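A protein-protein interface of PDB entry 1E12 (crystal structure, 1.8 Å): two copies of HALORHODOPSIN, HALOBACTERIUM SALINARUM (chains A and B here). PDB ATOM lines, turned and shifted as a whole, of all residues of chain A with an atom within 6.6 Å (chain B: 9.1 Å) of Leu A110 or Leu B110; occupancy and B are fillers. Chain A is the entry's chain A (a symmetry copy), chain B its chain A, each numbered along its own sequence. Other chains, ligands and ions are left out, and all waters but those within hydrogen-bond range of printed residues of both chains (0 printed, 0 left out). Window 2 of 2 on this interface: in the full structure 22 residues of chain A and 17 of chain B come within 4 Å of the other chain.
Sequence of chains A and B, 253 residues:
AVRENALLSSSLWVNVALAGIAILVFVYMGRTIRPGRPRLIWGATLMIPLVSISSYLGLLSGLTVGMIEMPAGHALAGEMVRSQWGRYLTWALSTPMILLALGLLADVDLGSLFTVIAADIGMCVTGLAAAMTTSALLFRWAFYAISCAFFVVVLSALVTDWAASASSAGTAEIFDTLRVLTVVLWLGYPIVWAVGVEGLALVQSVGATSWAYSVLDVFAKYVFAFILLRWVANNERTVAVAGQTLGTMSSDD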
ATOM      1  N   LEU A 100      13.947  -0.936   0.294  1.00  0.00           N
ATOM      2  CA  LEU A 100      13.302   0.296  -0.207  1.00  0.00           C
ATOM      3  C   LEU A 100      12.545  -0.012  -1.521  1.00  0.00           C
ATOM      4  O   LEU A 100      11.397   0.378  -1.707  1.00  0.00           O
ATOM      5  CB  LEU A 100      14.390   1.349  -0.458  1.00  0.00           C
ATOM      6  CG  LEU A 100      14.018   2.601  -1.267  1.00  0.00           C
ATOM      7  CD1 LEU A 100      12.932   3.316  -0.502  1.00  0.00           C
ATOM      8  CD2 LEU A 100      15.235   3.496  -1.463  1.00  0.00           C
ATOM      9  N   VAL A 108       4.220   0.552   0.952  1.00  0.00           N
ATOM     10  CA  VAL A 108       4.023   0.473   2.405  1.00  0.00           C
ATOM     11  C   VAL A 108       4.088   1.838   3.093  1.00  0.00           C
ATOM     12  O   VAL A 108       4.622   2.775   2.539  1.00  0.00           O
ATOM     13  CB  VAL A 108       5.080  -0.500   3.039  1.00  0.00           C
ATOM     14  CG1 VAL A 108       5.032  -1.844   2.335  1.00  0.00           C
ATOM     15  CG2 VAL A 108       6.446   0.090   2.947  1.00  0.00           C
ATOM     16  N   ASP A 109       3.551   1.980   4.304  1.00  0.00           N
ATOM     17  CA  ASP A 109       3.686   3.294   4.926  1.00  0.00           C
ATOM     18  C   ASP A 109       5.105   3.357   5.412  1.00  0.00           C
ATOM     19  O   ASP A 109       5.694   2.330   5.795  1.00  0.00           O
ATOM     20  CB  ASP A 109       2.674   3.506   6.061  1.00  0.00           C
ATOM     21  CG  ASP A 109       2.601   2.339   7.011  1.00  0.00           C
ATOM     22  OD1 ASP A 109       1.836   1.393   6.696  1.00  0.00           O
ATOM     23  OD2 ASP A 109       3.296   2.369   8.063  1.00  0.00           O
ATOM     24  N   LEU A 110       5.681   4.553   5.383  1.00  0.00           N
ATOM     25  CA  LEU A 110       7.056   4.658   5.788  1.00  0.00           C
ATOM     26  C   LEU A 110       7.282   4.333   7.252  1.00  0.00           C
ATOM     27  O   LEU A 110       8.434   4.201   7.677  1.00  0.00           O
ATOM     28  CB  LEU A 110       7.643   6.028   5.438  1.00  0.00           C
ATOM     29  CG  LEU A 110       9.155   5.812   5.183  1.00  0.00           C
ATOM     30  CD1 LEU A 110       9.472   6.136   3.698  1.00  0.00           C
ATOM     31  CD2 LEU A 110       9.988   6.649   6.121  1.00  0.00           C
ATOM     32  N   GLY A 111       6.199   4.233   8.024  1.00  0.00           N
ATOM     33  CA  GLY A 111       6.342   3.841   9.420  1.00  0.00           C
ATOM     34  C   GLY A 111       6.886   2.407   9.406  1.00  0.00           C
ATOM     35  O   GLY A 111       7.854   2.067  10.077  1.00  0.00           O
ATOM     36  N   SER A 112       6.249   1.578   8.590  1.00  0.00           N
ATOM     37  CA  SER A 112       6.652   0.184   8.411  1.00  0.00           C
ATOM     38  C   SER A 112       8.017   0.093   7.706  1.00  0.00           C
ATOM     39  O   SER A 112       8.861  -0.728   8.068  1.00  0.00           O
ATOM     40  CB  SER A 112       5.616  -0.531   7.559  1.00  0.00           C
ATOM     41  OG  SER A 112       5.954  -1.895   7.421  1.00  0.00           O
ATOM     42  N   LEU A 113       8.233   0.934   6.699  1.00  0.00           N
ATOM     43  CA  LEU A 113       9.496   0.885   5.975  1.00  0.00           C
ATOM     44  C   LEU A 113      10.667   1.276   6.851  1.00  0.00           C
ATOM     45  O   LEU A 113      11.739   0.692   6.787  1.00  0.00           O
ATOM     46  CB  LEU A 113       9.462   1.799   4.739  1.00  0.00           C
ATOM     47  CG  LEU A 113      10.828   1.806   4.037  1.00  0.00           C
ATOM     48  CD1 LEU A 113      10.948   0.509   3.243  1.00  0.00           C
ATOM     49  CD2 LEU A 113      10.987   3.012   3.131  1.00  0.00           C
ATOM     50  N   PHE A 114      10.468   2.299   7.660  1.00  0.00           N
ATOM     51  CA  PHE A 114      11.509   2.760   8.558  1.00  0.00           C
ATOM     52  C   PHE A 114      11.807   1.670   9.600  1.00  0.00           C
ATOM     53  O   PHE A 114      12.966   1.406   9.932  1.00  0.00           O
ATOM     54  CB  PHE A 114      11.053   4.041   9.278  1.00  0.00           C
ATOM     55  CG  PHE A 114      12.185   4.883   9.764  1.00  0.00           C
ATOM     56  CD1 PHE A 114      13.040   4.416  10.761  1.00  0.00           C
ATOM     57  CD2 PHE A 114      12.446   6.126   9.176  1.00  0.00           C
ATOM     58  CE1 PHE A 114      14.161   5.166  11.168  1.00  0.00           C
ATOM     59  CE2 PHE A 114      13.559   6.895   9.563  1.00  0.00           C
ATOM     60  CZ  PHE A 114      14.425   6.412  10.563  1.00  0.00           C
ATOM     61  N   THR A 115      10.760   1.042  10.109  1.00  0.00           N
ATOM     62  CA  THR A 115      10.942   0.020  11.134  1.00  0.00           C
ATOM     63  C   THR A 115      11.719  -1.179  10.546  1.00  0.00           C
ATOM     64  O   THR A 115      12.615  -1.698  11.175  1.00  0.00           O
ATOM     65  CB  THR A 115       9.577  -0.449  11.662  1.00  0.00           C
ATOM     66  OG1 THR A 115       8.822   0.687  12.130  1.00  0.00           O
ATOM     67  CG2 THR A 115       9.770  -1.429  12.814  1.00  0.00           C
ATOM     68  N   LEU B  40       3.646  -2.713  14.452  1.00  0.00           N
ATOM     69  CA  LEU B  40       4.932  -2.014  14.181  1.00  0.00           C
ATOM     70  C   LEU B  40       5.545  -1.560  15.515  1.00  0.00           C
ATOM     71  O   LEU B  40       6.727  -1.769  15.761  1.00  0.00           O
ATOM     72  CB  LEU B  40       4.759  -0.776  13.290  1.00  0.00           C
ATOM     73  CG  LEU B  40       4.249  -1.112  11.886  1.00  0.00           C
ATOM     74  CD1 LEU B  40       4.090   0.210  11.068  1.00  0.00           C
ATOM     75  CD2 LEU B  40       5.217  -2.130  11.204  1.00  0.00           C
ATOM     76  N   LEU B 100      11.565   6.266  17.234  1.00  0.00           N
ATOM     77  CA  LEU B 100      10.646   5.642  16.258  1.00  0.00           C
ATOM     78  C   LEU B 100       9.381   5.133  16.987  1.00  0.00           C
ATOM     79  O   LEU B 100       8.255   5.359  16.556  1.00  0.00           O
ATOM     80  CB  LEU B 100      11.374   4.473  15.581  1.00  0.00           C
ATOM     81  CG  LEU B 100      10.543   3.477  14.757  1.00  0.00           C
ATOM     82  CD1 LEU B 100       9.901   4.257  13.637  1.00  0.00           C
ATOM     83  CD2 LEU B 100      11.424   2.359  14.216  1.00  0.00           C
ATOM     84  N   GLY B 103       7.305   8.037  17.931  1.00  0.00           N
ATOM     85  CA  GLY B 103       6.723   8.719  16.769  1.00  0.00           C
ATOM     86  C   GLY B 103       5.576   7.903  16.164  1.00  0.00           C
ATOM     87  O   GLY B 103       4.616   8.475  15.622  1.00  0.00           O
ATOM     88  N   LEU B 104       5.707   6.578  16.194  1.00  0.00           N
ATOM     89  CA  LEU B 104       4.639   5.681  15.699  1.00  0.00           C
ATOM     90  C   LEU B 104       3.461   5.853  16.650  1.00  0.00           C
ATOM     91  O   LEU B 104       2.280   5.945  16.236  1.00  0.00           O
ATOM     92  CB  LEU B 104       5.107   4.228  15.729  1.00  0.00           C
ATOM     93  CG  LEU B 104       6.165   3.771  14.736  1.00  0.00           C
ATOM     94  CD1 LEU B 104       6.738   2.358  15.108  1.00  0.00           C
ATOM     95  CD2 LEU B 104       5.489   3.785  13.316  1.00  0.00           C
ATOM     96  N   ASP B 107       1.885   9.086  16.131  1.00  0.00           N
ATOM     97  CA  ASP B 107       1.454   9.119  14.734  1.00  0.00           C
ATOM     98  C   ASP B 107       1.997  10.380  14.034  1.00  0.00           C
ATOM     99  O   ASP B 107       1.270  11.075  13.299  1.00  0.00           O
ATOM    100  CB  ASP B 107      -0.086   9.102  14.719  1.00  0.00           C
ATOM    101  CG  ASP B 107      -0.661   9.154  13.339  1.00  0.00           C
ATOM    102  OD1 ASP B 107       0.016   8.664  12.407  1.00  0.00           O
ATOM    103  OD2 ASP B 107      -1.790   9.688  13.209  1.00  0.00           O
ATOM    104  N   VAL B 108       3.274  10.691  14.239  1.00  0.00           N
ATOM    105  CA  VAL B 108       3.812  11.928  13.659  1.00  0.00           C
ATOM    106  C   VAL B 108       4.074  11.820  12.156  1.00  0.00           C
ATOM    107  O   VAL B 108       4.185  10.731  11.632  1.00  0.00           O
ATOM    108  CB  VAL B 108       5.129  12.345  14.406  1.00  0.00           C
ATOM    109  CG1 VAL B 108       4.873  12.424  15.900  1.00  0.00           C
ATOM    110  CG2 VAL B 108       6.219  11.370  14.113  1.00  0.00           C
ATOM    111  N   ASP B 109       4.178  12.934  11.433  1.00  0.00           N
ATOM    112  CA  ASP B 109       4.473  12.764  10.014  1.00  0.00           C
ATOM    113  C   ASP B 109       5.938  12.440   9.950  1.00  0.00           C
ATOM    114  O   ASP B 109       6.732  12.908  10.787  1.00  0.00           O
ATOM    115  CB  ASP B 109       4.122  14.014   9.193  1.00  0.00           C
ATOM    116  CG  ASP B 109       4.625  15.289   9.817  1.00  0.00           C
ATOM    117  OD1 ASP B 109       3.895  15.827  10.687  1.00  0.00           O
ATOM    118  OD2 ASP B 109       5.735  15.752   9.439  1.00  0.00           O
ATOM    119  N   LEU B 110       6.314  11.617   8.979  1.00  0.00           N
ATOM    120  CA  LEU B 110       7.697  11.233   8.906  1.00  0.00           C
ATOM    121  C   LEU B 110       8.631  12.388   8.601  1.00  0.00           C
ATOM    122  O   LEU B 110       9.852  12.228   8.701  1.00  0.00           O
ATOM    123  CB  LEU B 110       7.912  10.083   7.917  1.00  0.00           C
ATOM    124  CG  LEU B 110       9.125   9.273   8.436  1.00  0.00           C
ATOM    125  CD1 LEU B 110       8.654   7.846   8.828  1.00  0.00           C
ATOM    126  CD2 LEU B 110      10.225   9.227   7.405  1.00  0.00           C
ATOM    127  N   GLY B 111       8.070  13.532   8.206  1.00  0.00           N
ATOM    128  CA  GLY B 111       8.906  14.703   7.977  1.00  0.00           C
ATOM    129  C   GLY B 111       9.507  15.070   9.340  1.00  0.00           C
ATOM    130  O   GLY B 111      10.705  15.277   9.494  1.00  0.00           O
ATOM    131  N   SER B 112       8.635  15.114  10.339  1.00  0.00           N
ATOM    132  CA  SER B 112       9.029  15.403  11.717  1.00  0.00           C
ATOM    133  C   SER B 112       9.885  14.263  12.294  1.00  0.00           C
ATOM    134  O   SER B 112      10.871  14.504  12.992  1.00  0.00           O
ATOM    135  CB  SER B 112       7.783  15.557  12.572  1.00  0.00           C
ATOM    136  OG  SER B 112       8.137  15.895  13.896  1.00  0.00           O
ATOM    137  N   LEU B 113       9.509  13.020  12.006  1.00  0.00           N
ATOM    138  CA  LEU B 113      10.264  11.894  12.540  1.00  0.00           C
ATOM    139  C   LEU B 113      11.670  11.839  11.982  1.00  0.00           C
ATOM    140  O   LEU B 113      12.627  11.543  12.683  1.00  0.00           O
ATOM    141  CB  LEU B 113       9.552  10.562  12.249  1.00  0.00           C
ATOM    142  CG  LEU B 113      10.401   9.380  12.739  1.00  0.00           C
ATOM    143  CD1 LEU B 113      10.243   9.292  14.253  1.00  0.00           C
ATOM    144  CD2 LEU B 113       9.990   8.081  12.074  1.00  0.00           C
ATOM    145  N   PHE B 114      11.792  12.098  10.694  1.00  0.00           N
ATOM    146  CA  PHE B 114      13.089  12.091  10.046  1.00  0.00           C
ATOM    147  C   PHE B 114      13.954  13.227  10.614  1.00  0.00           C
ATOM    148  O   PHE B 114      15.147  13.051  10.873  1.00  0.00           O
ATOM    149  CB  PHE B 114      12.920  12.288   8.530  1.00  0.00           C
ATOM    150  CG  PHE B 114      14.062  11.754   7.731  1.00  0.00           C
ATOM    151  CD1 PHE B 114      15.332  12.319   7.842  1.00  0.00           C
ATOM    152  CD2 PHE B 114      13.890  10.633   6.912  1.00  0.00           C
ATOM    153  CE1 PHE B 114      16.435  11.771   7.159  1.00  0.00           C
ATOM    154  CE2 PHE B 114      14.974  10.065   6.218  1.00  0.00           C
ATOM    155  CZ  PHE B 114      16.256  10.635   6.344  1.00  0.00           C
ATOM    156  N   THR B 115      13.346  14.386  10.807  1.00  0.00           N
ATOM    157  CA  THR B 115      14.095  15.536  11.306  1.00  0.00           C
ATOM    158  C   THR B 115      14.599  15.251  12.738  1.00  0.00           C
ATOM    159  O   THR B 115      15.731  15.538  13.060  1.00  0.00           O
ATOM    160  CB  THR B 115      13.205  16.788  11.304  1.00  0.00           C
ATOM    161  OG1 THR B 115      12.667  16.998   9.982  1.00  0.00           O
ATOM    162  CG2 THR B 115      14.021  18.009  11.712  1.00  0.00           C
ATOM    163  N   VAL B 116      13.743  14.669  13.580  1.00  0.00           N
ATOM    164  CA  VAL B 116      14.142  14.367  14.966  1.00  0.00           C
ATOM    165  C   VAL B 116      15.196  13.274  15.028  1.00  0.00           C
ATOM    166  O   VAL B 116      16.145  13.366  15.815  1.00  0.00           O
ATOM    167  CB  VAL B 116      12.892  14.000  15.827  1.00  0.00           C
ATOM    168  CG1 VAL B 116      13.322  13.534  17.216  1.00  0.00           C
ATOM    169  CG2 VAL B 116      11.962  15.239  15.923  1.00  0.00           C
ATOM    170  N   ILE B 117      15.063  12.223  14.208  1.00  0.00           N
ATOM    171  CA  ILE B 117      16.091  11.168  14.203  1.00  0.00           C
ATOM    172  C   ILE B 117      17.406  11.714  13.694  1.00  0.00           C
ATOM    173  O   ILE B 117      18.474  11.329  14.178  1.00  0.00           O
ATOM    174  CB  ILE B 117      15.674   9.943  13.349  1.00  0.00           C
ATOM    175  CG1 ILE B 117      14.596   9.187  14.131  1.00  0.00           C
ATOM    176  CG2 ILE B 117      16.913   9.023  13.035  1.00  0.00           C
ATOM    177  CD1 ILE B 117      13.742   8.259  13.280  1.00  0.00           C
ATOM    178  N   ALA B 118      17.327  12.634  12.725  1.00  0.00           N
ATOM    179  CA  ALA B 118      18.578  13.254  12.219  1.00  0.00           C
ATOM    180  C   ALA B 118      19.263  14.018  13.372  1.00  0.00           C
ATOM    181  O   ALA B 118      20.464  13.903  13.581  1.00  0.00           O
ATOM    182  CB  ALA B 118      18.274  14.238  11.080  1.00  0.00           C
ATOM    183  N   ASP B 161       6.071  19.688  19.331  1.00  0.00           N
ATOM    184  CA  ASP B 161       5.461  19.165  18.108  1.00  0.00           C
ATOM    185  C   ASP B 161       4.848  17.771  18.189  1.00  0.00           C
ATOM    186  O   ASP B 161       3.727  17.545  17.729  1.00  0.00           O
ATOM    187  CB  ASP B 161       6.447  19.127  16.950  1.00  0.00           C
ATOM    188  CG  ASP B 161       5.820  18.529  15.698  1.00  0.00           C
ATOM    189  OD1 ASP B 161       4.576  18.339  15.717  1.00  0.00           O
ATOM    190  OD2 ASP B 161       6.532  18.256  14.705  1.00  0.00           O
ATOM    191  N   TRP B 162       5.599  16.820  18.728  1.00  0.00           N
ATOM    192  CA  TRP B 162       5.100  15.467  18.799  1.00  0.00           C
ATOM    193  C   TRP B 162       3.838  15.328  19.649  1.00  0.00           C
ATOM    194  O   TRP B 162       2.948  14.546  19.308  1.00  0.00           O
ATOM    195  CB  TRP B 162       6.225  14.543  19.255  1.00  0.00           C
ATOM    196  CG  TRP B 162       7.189  14.278  18.129  1.00  0.00           C
ATOM    197  CD1 TRP B 162       7.371  15.055  17.010  1.00  0.00           C
ATOM    198  CD2 TRP B 162       8.071  13.160  17.987  1.00  0.00           C
ATOM    199  NE1 TRP B 162       8.299  14.487  16.189  1.00  0.00           N
ATOM    200  CE2 TRP B 162       8.753  13.322  16.758  1.00  0.00           C
ATOM    201  CE3 TRP B 162       8.352  12.036  18.776  1.00  0.00           C
ATOM    202  CZ2 TRP B 162       9.688  12.411  16.295  1.00  0.00           C
ATOM    203  CZ3 TRP B 162       9.285  11.125  18.320  1.00  0.00           C
ATOM    204  CH2 TRP B 162       9.950  11.312  17.082  1.00  0.00           C
ATOM    205  N   SER B 165       0.767  15.861  17.659  1.00  0.00           N
ATOM    206  CA  SER B 165       0.445  14.705  16.840  1.00  0.00           C
ATOM    207  C   SER B 165      -0.285  13.633  17.691  1.00  0.00           C
ATOM    208  O   SER B 165      -1.266  13.039  17.250  1.00  0.00           O
ATOM    209  CB  SER B 165       1.750  14.166  16.252  1.00  0.00           C
ATOM    210  OG  SER B 165       1.526  13.531  15.024  1.00  0.00           O
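Of the 9 printed residues of chain A, 6 touch a printed residue of chain B. Of the 19 printed residues of chain B, 5 touch a printed residue of chain A. Among the printed residues, 7 pairs touch across the chains. Among the printed residues, no Asp or Glu carboxylate lies within 4 Å of a Lys or Arg side-chain nitrogen of the other chain.
Leu B110 touches its own counterpart, Leu A110. Thr A115 touches Leu B100, but with the chains exchanged Leu A100 does not touch Thr B115 (15.8 Å). Positions printed for both chains: 100, 108, 109, 110, 111, 112, 113, 114 and 115. Of the 7 pairs that touch across the chains among the printed residues, 1 has its exchanged pair printed and touching as well.
Leu A110 touches one residue of chain B. Leu B110 touches one residue of chain A. Of the printed residues of chain A, Leu B40 touches Asp A109, Gly A111 and Ser A112. Of the printed residues of chain A, Leu B104 touches Gly A111 (3.99 Å). Printed residues of chain B within 4 Å of Gly A111: Leu B40 and Leu B104. Of the printed residues of chain B, Asp A109 touches Leu B40 (3.8 Å). Leu A100 touches none of the printed residues of chain B. The nearest residue of chain B that does not touch Leu A110 is Phe B114 (5.6 Å). The nearest residue of chain A that does not touch Leu B110 is Phe A114 (4.2 Å). The nearest printed residue of chain B that does not touch Thr A115 is Leu B104 (4.0005 Å).
CD1 of Leu B40 touches OD2 of Asp A109 (3.8 Å). Leu B110 touches Leu A110 (CD2 to CD2, 2.9 Å). Gly A111 touches Leu B40. Gly A111 touches Leu B104. Ser A112 touches Leu B40 (N to CD1, 3.6 Å). CZ of Phe A114 touches CD1 of Ile B117, at 3.4 Å. Leu B100 touches Thr A115.
The side-chain carboxylate of Asp A109 sits close to the backbone NH of Gly A111 (3.5 Å). The side-chain carboxylate (OD2) of Asp A109 sits at hydrogen-bond distance from the backbone NH (N) of Ser A112 (3.1 Å). The backbone carbonyl oxygen (O) of Gly A111 is in hydrogen-bond range of the side-chain hydroxyl (OG1) of Thr A115 (2.7 Å).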
